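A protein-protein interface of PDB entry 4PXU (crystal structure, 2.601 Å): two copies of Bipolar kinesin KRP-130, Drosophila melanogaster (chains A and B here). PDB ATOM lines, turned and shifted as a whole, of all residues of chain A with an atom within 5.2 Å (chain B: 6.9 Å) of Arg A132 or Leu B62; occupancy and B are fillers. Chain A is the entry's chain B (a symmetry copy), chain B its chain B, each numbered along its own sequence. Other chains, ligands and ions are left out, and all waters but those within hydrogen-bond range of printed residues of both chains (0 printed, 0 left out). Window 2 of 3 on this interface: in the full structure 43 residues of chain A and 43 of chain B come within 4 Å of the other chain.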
ATOM      1  N   THR A 128     -23.953  -4.767 -18.730  1.00  0.00           N
ATOM      2  CA  THR A 128     -23.986  -5.529 -19.971  1.00  0.00           C
ATOM      3  C   THR A 128     -22.644  -6.180 -20.257  1.00  0.00           C
ATOM      4  O   THR A 128     -22.573  -7.357 -20.595  1.00  0.00           O
ATOM      5  CB  THR A 128     -24.397  -4.629 -21.152  1.00  0.00           C
ATOM      6  OG1 THR A 128     -25.802  -4.367 -21.065  1.00  0.00           O
ATOM      7  CG2 THR A 128     -24.121  -5.315 -22.476  1.00  0.00           C
ATOM      8  N   ARG A 129     -21.577  -5.415 -20.080  1.00  0.00           N
ATOM      9  CA  ARG A 129     -20.233  -5.929 -20.286  1.00  0.00           C
ATOM     10  C   ARG A 129     -19.952  -7.118 -19.366  1.00  0.00           C
ATOM     11  O   ARG A 129     -19.292  -8.075 -19.767  1.00  0.00           O
ATOM     12  CB  ARG A 129     -19.205  -4.821 -20.060  1.00  0.00           C
ATOM     13  CG  ARG A 129     -17.771  -5.274 -20.222  1.00  0.00           C
ATOM     14  CD  ARG A 129     -16.847  -4.080 -20.322  1.00  0.00           C
ATOM     15  NE  ARG A 129     -16.868  -3.230 -19.129  1.00  0.00           N
ATOM     16  CZ  ARG A 129     -17.392  -2.008 -19.104  1.00  0.00           C
ATOM     17  NH1 ARG A 129     -17.947  -1.504 -20.207  1.00  0.00           N
ATOM     18  NH2 ARG A 129     -17.372  -1.295 -17.981  1.00  0.00           N
ATOM     19  N   ASN A 130     -20.477  -7.063 -18.144  1.00  0.00           N
ATOM     20  CA  ASN A 130     -20.304  -8.147 -17.182  1.00  0.00           C
ATOM     21  C   ASN A 130     -21.000  -9.428 -17.610  1.00  0.00           C
ATOM     22  O   ASN A 130     -20.478 -10.524 -17.421  1.00  0.00           O
ATOM     23  CB  ASN A 130     -20.851  -7.747 -15.821  1.00  0.00           C
ATOM     24  CG  ASN A 130     -20.002  -6.722 -15.137  1.00  0.00           C
ATOM     25  OD1 ASN A 130     -18.857  -6.488 -15.519  1.00  0.00           O
ATOM     26  ND2 ASN A 130     -20.554  -6.111 -14.097  1.00  0.00           N
ATOM     27  N   HIS A 131     -22.187  -9.277 -18.181  1.00  0.00           N
ATOM     28  CA  HIS A 131     -22.937 -10.413 -18.672  1.00  0.00           C
ATOM     29  C   HIS A 131     -22.197 -11.045 -19.830  1.00  0.00           C
ATOM     30  O   HIS A 131     -22.097 -12.272 -19.913  1.00  0.00           O
ATOM     31  CB  HIS A 131     -24.346  -9.995 -19.082  1.00  0.00           C
ATOM     32  CG  HIS A 131     -25.158  -9.442 -17.953  1.00  0.00           C
ATOM     33  ND1 HIS A 131     -25.270 -10.081 -16.733  1.00  0.00           N
ATOM     34  CD2 HIS A 131     -25.882  -8.303 -17.842  1.00  0.00           C
ATOM     35  CE1 HIS A 131     -26.034  -9.365 -15.930  1.00  0.00           C
ATOM     36  NE2 HIS A 131     -26.420  -8.278 -16.579  1.00  0.00           N
ATOM     37  N   ARG A 132     -21.659 -10.209 -20.714  1.00  0.00           N
ATOM     38  CA  ARG A 132     -20.958 -10.725 -21.888  1.00  0.00           C
ATOM     39  C   ARG A 132     -19.689 -11.454 -21.495  1.00  0.00           C
ATOM     40  O   ARG A 132     -19.348 -12.484 -22.084  1.00  0.00           O
ATOM     41  CB  ARG A 132     -20.629  -9.602 -22.871  1.00  0.00           C
ATOM     42  CG  ARG A 132     -21.865  -9.005 -23.514  1.00  0.00           C
ATOM     43  CD  ARG A 132     -21.512  -8.126 -24.696  1.00  0.00           C
ATOM     44  NE  ARG A 132     -22.700  -7.499 -25.271  1.00  0.00           N
ATOM     45  CZ  ARG A 132     -22.683  -6.667 -26.310  1.00  0.00           C
ATOM     46  NH1 ARG A 132     -21.533  -6.368 -26.901  1.00  0.00           N
ATOM     47  NH2 ARG A 132     -23.814  -6.135 -26.760  1.00  0.00           N
ATOM     48  N   ILE A 133     -19.011 -10.941 -20.475  1.00  0.00           N
ATOM     49  CA  ILE A 133     -17.800 -11.585 -19.989  1.00  0.00           C
ATOM     50  C   ILE A 133     -18.151 -12.919 -19.337  1.00  0.00           C
ATOM     51  O   ILE A 133     -17.452 -13.916 -19.524  1.00  0.00           O
ATOM     52  CB  ILE A 133     -17.026 -10.665 -19.020  1.00  0.00           C
ATOM     53  CG1 ILE A 133     -16.458  -9.479 -19.810  1.00  0.00           C
ATOM     54  CG2 ILE A 133     -15.894 -11.414 -18.324  1.00  0.00           C
ATOM     55  CD1 ILE A 133     -15.451  -8.637 -19.068  1.00  0.00           C
ATOM     56  N   ASP A 134     -19.255 -12.950 -18.602  1.00  0.00           N
ATOM     57  CA  ASP A 134     -19.675 -14.185 -17.965  1.00  0.00           C
ATOM     58  C   ASP A 134     -20.070 -15.231 -19.003  1.00  0.00           C
ATOM     59  O   ASP A 134     -19.789 -16.421 -18.831  1.00  0.00           O
ATOM     60  CB  ASP A 134     -20.820 -13.915 -16.999  1.00  0.00           C
ATOM     61  CG  ASP A 134     -20.353 -13.196 -15.753  1.00  0.00           C
ATOM     62  OD1 ASP A 134     -19.120 -13.034 -15.599  1.00  0.00           O
ATOM     63  OD2 ASP A 134     -21.208 -12.811 -14.926  1.00  0.00           O
ATOM     64  N   ASP A 135     -20.704 -14.786 -20.085  1.00  0.00           N
ATOM     65  CA  ASP A 135     -21.050 -15.690 -21.179  1.00  0.00           C
ATOM     66  C   ASP A 135     -19.821 -16.313 -21.802  1.00  0.00           C
ATOM     67  O   ASP A 135     -19.794 -17.511 -22.081  1.00  0.00           O
ATOM     68  CB  ASP A 135     -21.844 -14.968 -22.264  1.00  0.00           C
ATOM     69  CG  ASP A 135     -23.295 -14.834 -21.911  1.00  0.00           C
ATOM     70  OD1 ASP A 135     -23.769 -15.624 -21.063  1.00  0.00           O
ATOM     71  OD2 ASP A 135     -23.960 -13.944 -22.481  1.00  0.00           O
ATOM     72  N   ILE A 136     -18.804 -15.492 -22.016  1.00  0.00           N
ATOM     73  CA  ILE A 136     -17.565 -15.966 -22.613  1.00  0.00           C
ATOM     74  C   ILE A 136     -16.868 -16.923 -21.638  1.00  0.00           C
ATOM     75  O   ILE A 136     -16.326 -17.948 -22.051  1.00  0.00           O
ATOM     76  CB  ILE A 136     -16.637 -14.786 -22.983  1.00  0.00           C
ATOM     77  CG1 ILE A 136     -17.350 -13.826 -23.938  1.00  0.00           C
ATOM     78  CG2 ILE A 136     -15.348 -15.288 -23.585  1.00  0.00           C
ATOM     79  CD1 ILE A 136     -16.574 -12.567 -24.240  1.00  0.00           C
ATOM     80  N   LYS A 137     -16.898 -16.599 -20.345  1.00  0.00           N
ATOM     81  CA  LYS A 137     -16.351 -17.495 -19.325  1.00  0.00           C
ATOM     82  C   LYS A 137     -17.075 -18.838 -19.348  1.00  0.00           C
ATOM     83  O   LYS A 137     -16.446 -19.897 -19.299  1.00  0.00           O
ATOM     84  CB  LYS A 137     -16.472 -16.878 -17.931  1.00  0.00           C
ATOM     85  CG  LYS A 137     -15.427 -15.826 -17.575  1.00  0.00           C
ATOM     86  CD  LYS A 137     -15.689 -15.298 -16.162  1.00  0.00           C
ATOM     87  CE  LYS A 137     -14.742 -14.174 -15.766  1.00  0.00           C
ATOM     88  NZ  LYS A 137     -15.089 -13.614 -14.420  1.00  0.00           N
ATOM     89  N   LYS B  57     -16.513 -14.067 -32.370  1.00  0.00           N
ATOM     90  CA  LYS B  57     -17.735 -13.290 -32.553  1.00  0.00           C
ATOM     91  C   LYS B  57     -18.147 -12.619 -31.238  1.00  0.00           C
ATOM     92  O   LYS B  57     -18.533 -11.451 -31.225  1.00  0.00           O
ATOM     93  CB  LYS B  57     -18.871 -14.166 -33.081  1.00  0.00           C
ATOM     94  CG  LYS B  57     -20.195 -13.425 -33.233  1.00  0.00           C
ATOM     95  CD  LYS B  57     -21.318 -14.367 -33.631  1.00  0.00           C
ATOM     96  CE  LYS B  57     -22.651 -13.640 -33.715  1.00  0.00           C
ATOM     97  NZ  LYS B  57     -23.749 -14.578 -34.086  1.00  0.00           N
ATOM     98  N   LYS B  58     -18.087 -13.369 -30.139  1.00  0.00           N
ATOM     99  CA  LYS B  58     -18.354 -12.814 -28.812  1.00  0.00           C
ATOM    100  C   LYS B  58     -17.380 -11.698 -28.436  1.00  0.00           C
ATOM    101  O   LYS B  58     -17.778 -10.696 -27.827  1.00  0.00           O
ATOM    102  CB  LYS B  58     -18.298 -13.909 -27.744  1.00  0.00           C
ATOM    103  CG  LYS B  58     -19.340 -14.985 -27.895  1.00  0.00           C
ATOM    104  CD  LYS B  58     -20.730 -14.417 -27.694  1.00  0.00           C
ATOM    105  CE  LYS B  58     -21.749 -15.538 -27.585  1.00  0.00           C
ATOM    106  NZ  LYS B  58     -21.403 -16.475 -26.478  1.00  0.00           N
ATOM    107  N   LEU B  59     -16.107 -11.885 -28.783  1.00  0.00           N
ATOM    108  CA  LEU B  59     -15.071 -10.907 -28.463  1.00  0.00           C
ATOM    109  C   LEU B  59     -15.166  -9.694 -29.375  1.00  0.00           C
ATOM    110  O   LEU B  59     -14.692  -8.615 -29.026  1.00  0.00           O
ATOM    111  CB  LEU B  59     -13.675 -11.527 -28.577  1.00  0.00           C
ATOM    112  CG  LEU B  59     -13.208 -12.547 -27.536  1.00  0.00           C
ATOM    113  CD1 LEU B  59     -11.883 -13.158 -27.955  1.00  0.00           C
ATOM    114  CD2 LEU B  59     -13.056 -11.887 -26.182  1.00  0.00           C
ATOM    115  N   GLU B  60     -15.792  -9.863 -30.535  1.00  0.00           N
ATOM    116  CA  GLU B  60     -15.936  -8.749 -31.461  1.00  0.00           C
ATOM    117  C   GLU B  60     -16.935  -7.761 -30.904  1.00  0.00           C
ATOM    118  O   GLU B  60     -16.659  -6.563 -30.820  1.00  0.00           O
ATOM    119  CB  GLU B  60     -16.394  -9.220 -32.842  1.00  0.00           C
ATOM    120  CG  GLU B  60     -15.268  -9.643 -33.767  1.00  0.00           C
ATOM    121  CD  GLU B  60     -14.178  -8.597 -33.863  1.00  0.00           C
ATOM    122  OE1 GLU B  60     -14.473  -7.474 -34.326  1.00  0.00           O
ATOM    123  OE2 GLU B  60     -13.028  -8.893 -33.472  1.00  0.00           O
ATOM    124  N   GLN B  61     -18.092  -8.269 -30.496  1.00  0.00           N
ATOM    125  CA  GLN B  61     -19.149  -7.382 -30.040  1.00  0.00           C
ATOM    126  C   GLN B  61     -18.860  -6.835 -28.645  1.00  0.00           C
ATOM    127  O   GLN B  61     -19.301  -5.734 -28.305  1.00  0.00           O
ATOM    128  CB  GLN B  61     -20.505  -8.089 -30.072  1.00  0.00           C
ATOM    129  CG  GLN B  61     -20.695  -9.188 -29.061  1.00  0.00           C
ATOM    130  CD  GLN B  61     -22.089  -9.781 -29.149  1.00  0.00           C
ATOM    131  OE1 GLN B  61     -23.019  -9.304 -28.487  1.00  0.00           O
ATOM    132  NE2 GLN B  61     -22.250 -10.811 -29.985  1.00  0.00           N
ATOM    133  N   LEU B  62     -18.091  -7.582 -27.856  1.00  0.00           N
ATOM    134  CA  LEU B  62     -17.663  -7.096 -26.547  1.00  0.00           C
ATOM    135  C   LEU B  62     -16.721  -5.911 -26.722  1.00  0.00           C
ATOM    136  O   LEU B  62     -16.850  -4.893 -26.042  1.00  0.00           O
ATOM    137  CB  LEU B  62     -16.989  -8.204 -25.742  1.00  0.00           C
ATOM    138  CG  LEU B  62     -16.379  -7.827 -24.389  1.00  0.00           C
ATOM    139  CD1 LEU B  62     -17.441  -7.336 -23.420  1.00  0.00           C
ATOM    140  CD2 LEU B  62     -15.653  -9.031 -23.804  1.00  0.00           C
ATOM    141  N   GLY B  63     -15.791  -6.038 -27.662  1.00  0.00           N
ATOM    142  CA  GLY B  63     -14.852  -4.971 -27.948  1.00  0.00           C
ATOM    143  C   GLY B  63     -15.524  -3.828 -28.679  1.00  0.00           C
ATOM    144  O   GLY B  63     -14.958  -2.743 -28.802  1.00  0.00           O
ATOM    145  N   ALA B  64     -16.743  -4.065 -29.157  1.00  0.00           N
ATOM    146  CA  ALA B  64     -17.488  -3.035 -29.876  1.00  0.00           C
ATOM    147  C   ALA B  64     -18.108  -2.037 -28.896  1.00  0.00           C
ATOM    148  O   ALA B  64     -18.547  -0.960 -29.287  1.00  0.00           O
ATOM    149  CB  ALA B  64     -18.559  -3.658 -30.744  1.00  0.00           C
ATOM    150  N   MET B  65     -18.124  -2.402 -27.617  1.00  0.00           N
ATOM    151  CA  MET B  65     -18.687  -1.555 -26.572  1.00  0.00           C
ATOM    152  C   MET B  65     -17.749  -0.401 -26.267  1.00  0.00           C
ATOM    153  O   MET B  65     -18.133   0.585 -25.637  1.00  0.00           O
ATOM    154  CB  MET B  65     -18.943  -2.360 -25.300  1.00  0.00           C
ATOM    155  CG  MET B  65     -19.822  -3.557 -25.496  1.00  0.00           C
ATOM    156  SD  MET B  65     -20.232  -4.286 -23.915  1.00  0.00           S
ATOM    157  CE  MET B  65     -21.384  -3.071 -23.276  1.00  0.00           C
ATOM    158  N   SER B  66     -16.508  -0.551 -26.708  1.00  0.00           N
ATOM    159  CA  SER B  66     -15.469   0.420 -26.435  1.00  0.00           C
ATOM    160  C   SER B  66     -15.827   1.782 -27.014  1.00  0.00           C
ATOM    161  O   SER B  66     -15.574   2.815 -26.388  1.00  0.00           O
ATOM    162  CB  SER B  66     -14.134  -0.060 -27.000  1.00  0.00           C
ATOM    163  OG  SER B  66     -13.088   0.795 -26.580  1.00  0.00           O
ATOM    164  N   ASP B  69     -18.626   3.555 -25.116  1.00  0.00           N
ATOM    165  CA  ASP B  69     -17.997   3.896 -23.841  1.00  0.00           C
ATOM    166  C   ASP B  69     -17.168   5.160 -23.994  1.00  0.00           C
ATOM    167  O   ASP B  69     -17.193   6.037 -23.136  1.00  0.00           O
ATOM    168  CB  ASP B  69     -17.116   2.746 -23.336  1.00  0.00           C
ATOM    169  CG  ASP B  69     -17.922   1.583 -22.763  1.00  0.00           C
ATOM    170  OD1 ASP B  69     -19.146   1.727 -22.571  1.00  0.00           O
ATOM    171  OD2 ASP B  69     -17.332   0.502 -22.542  1.00  0.00           O
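Printed residues of chain B within 4 Å of Thr A128: Met B65 (3.6 Å).
Arg A132 touches just these residues of chain B: Gln B61, Leu B62 and Met B65.
Glu B60 touches none of the printed residues of chain A.
Printed residues of chain A within 4 Å of Gln B61: Arg A132 (2.7 Å).
Of chain A, only Arg A129 (3.8 Å), Arg A132 (3.8 Å) and Ile A136 (3.7 Å) come within 4 Å of Leu B62.
The guanidinium group (NH1) of Arg A132 lies within hydrogen-bond range of the backbone carbonyl oxygen (O) of Gln B61 (2.7 Å).
The guanidinium group (NH1) of Arg A129 lies within salt-bridge range of the side-chain carboxylate (OD2) of Asp B69 (3.1 Å).
No position is printed for both chains.
Of the 9 pairs that touch across the chains among the printed residues, none has its exchanged pair printed and touching as well.
Of the 10 printed residues of chain A, 4 touch a printed residue of chain B.
Hydrophobic or aromatic side chains of chain A that line the printed part of chain B: Ile A136.
Along chain A the printed residues that touch a printed residue of chain B span positions 128 to 136.
Hydrophobic or aromatic side chains of chain B within 4 Å of the printed part of chain A: Leu B62 and Met B65.
Along chain B the printed residues that touch a printed residue of chain A span positions 58 to 69.
Among the printed residues, Asp or Glu carboxylates within 4 Å of a Lys or Arg side-chain nitrogen of the other chain: Arg A129 with Asp B69 (3.1 Å).
Among the printed residues, merely in contact across the chains: Arg A132 with Met B65 (3.6 Å), Thr A128 with Met B65 (3.6 Å), Ile A136 with Leu B62 (3.7 Å), Arg A132 with Leu B62 (3.8 Å), Arg A129 with Leu B62 (3.8 Å), Ile A136 with Lys B58 (3.9 Å) and Arg A129 with Met B65 (3.97 Å).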
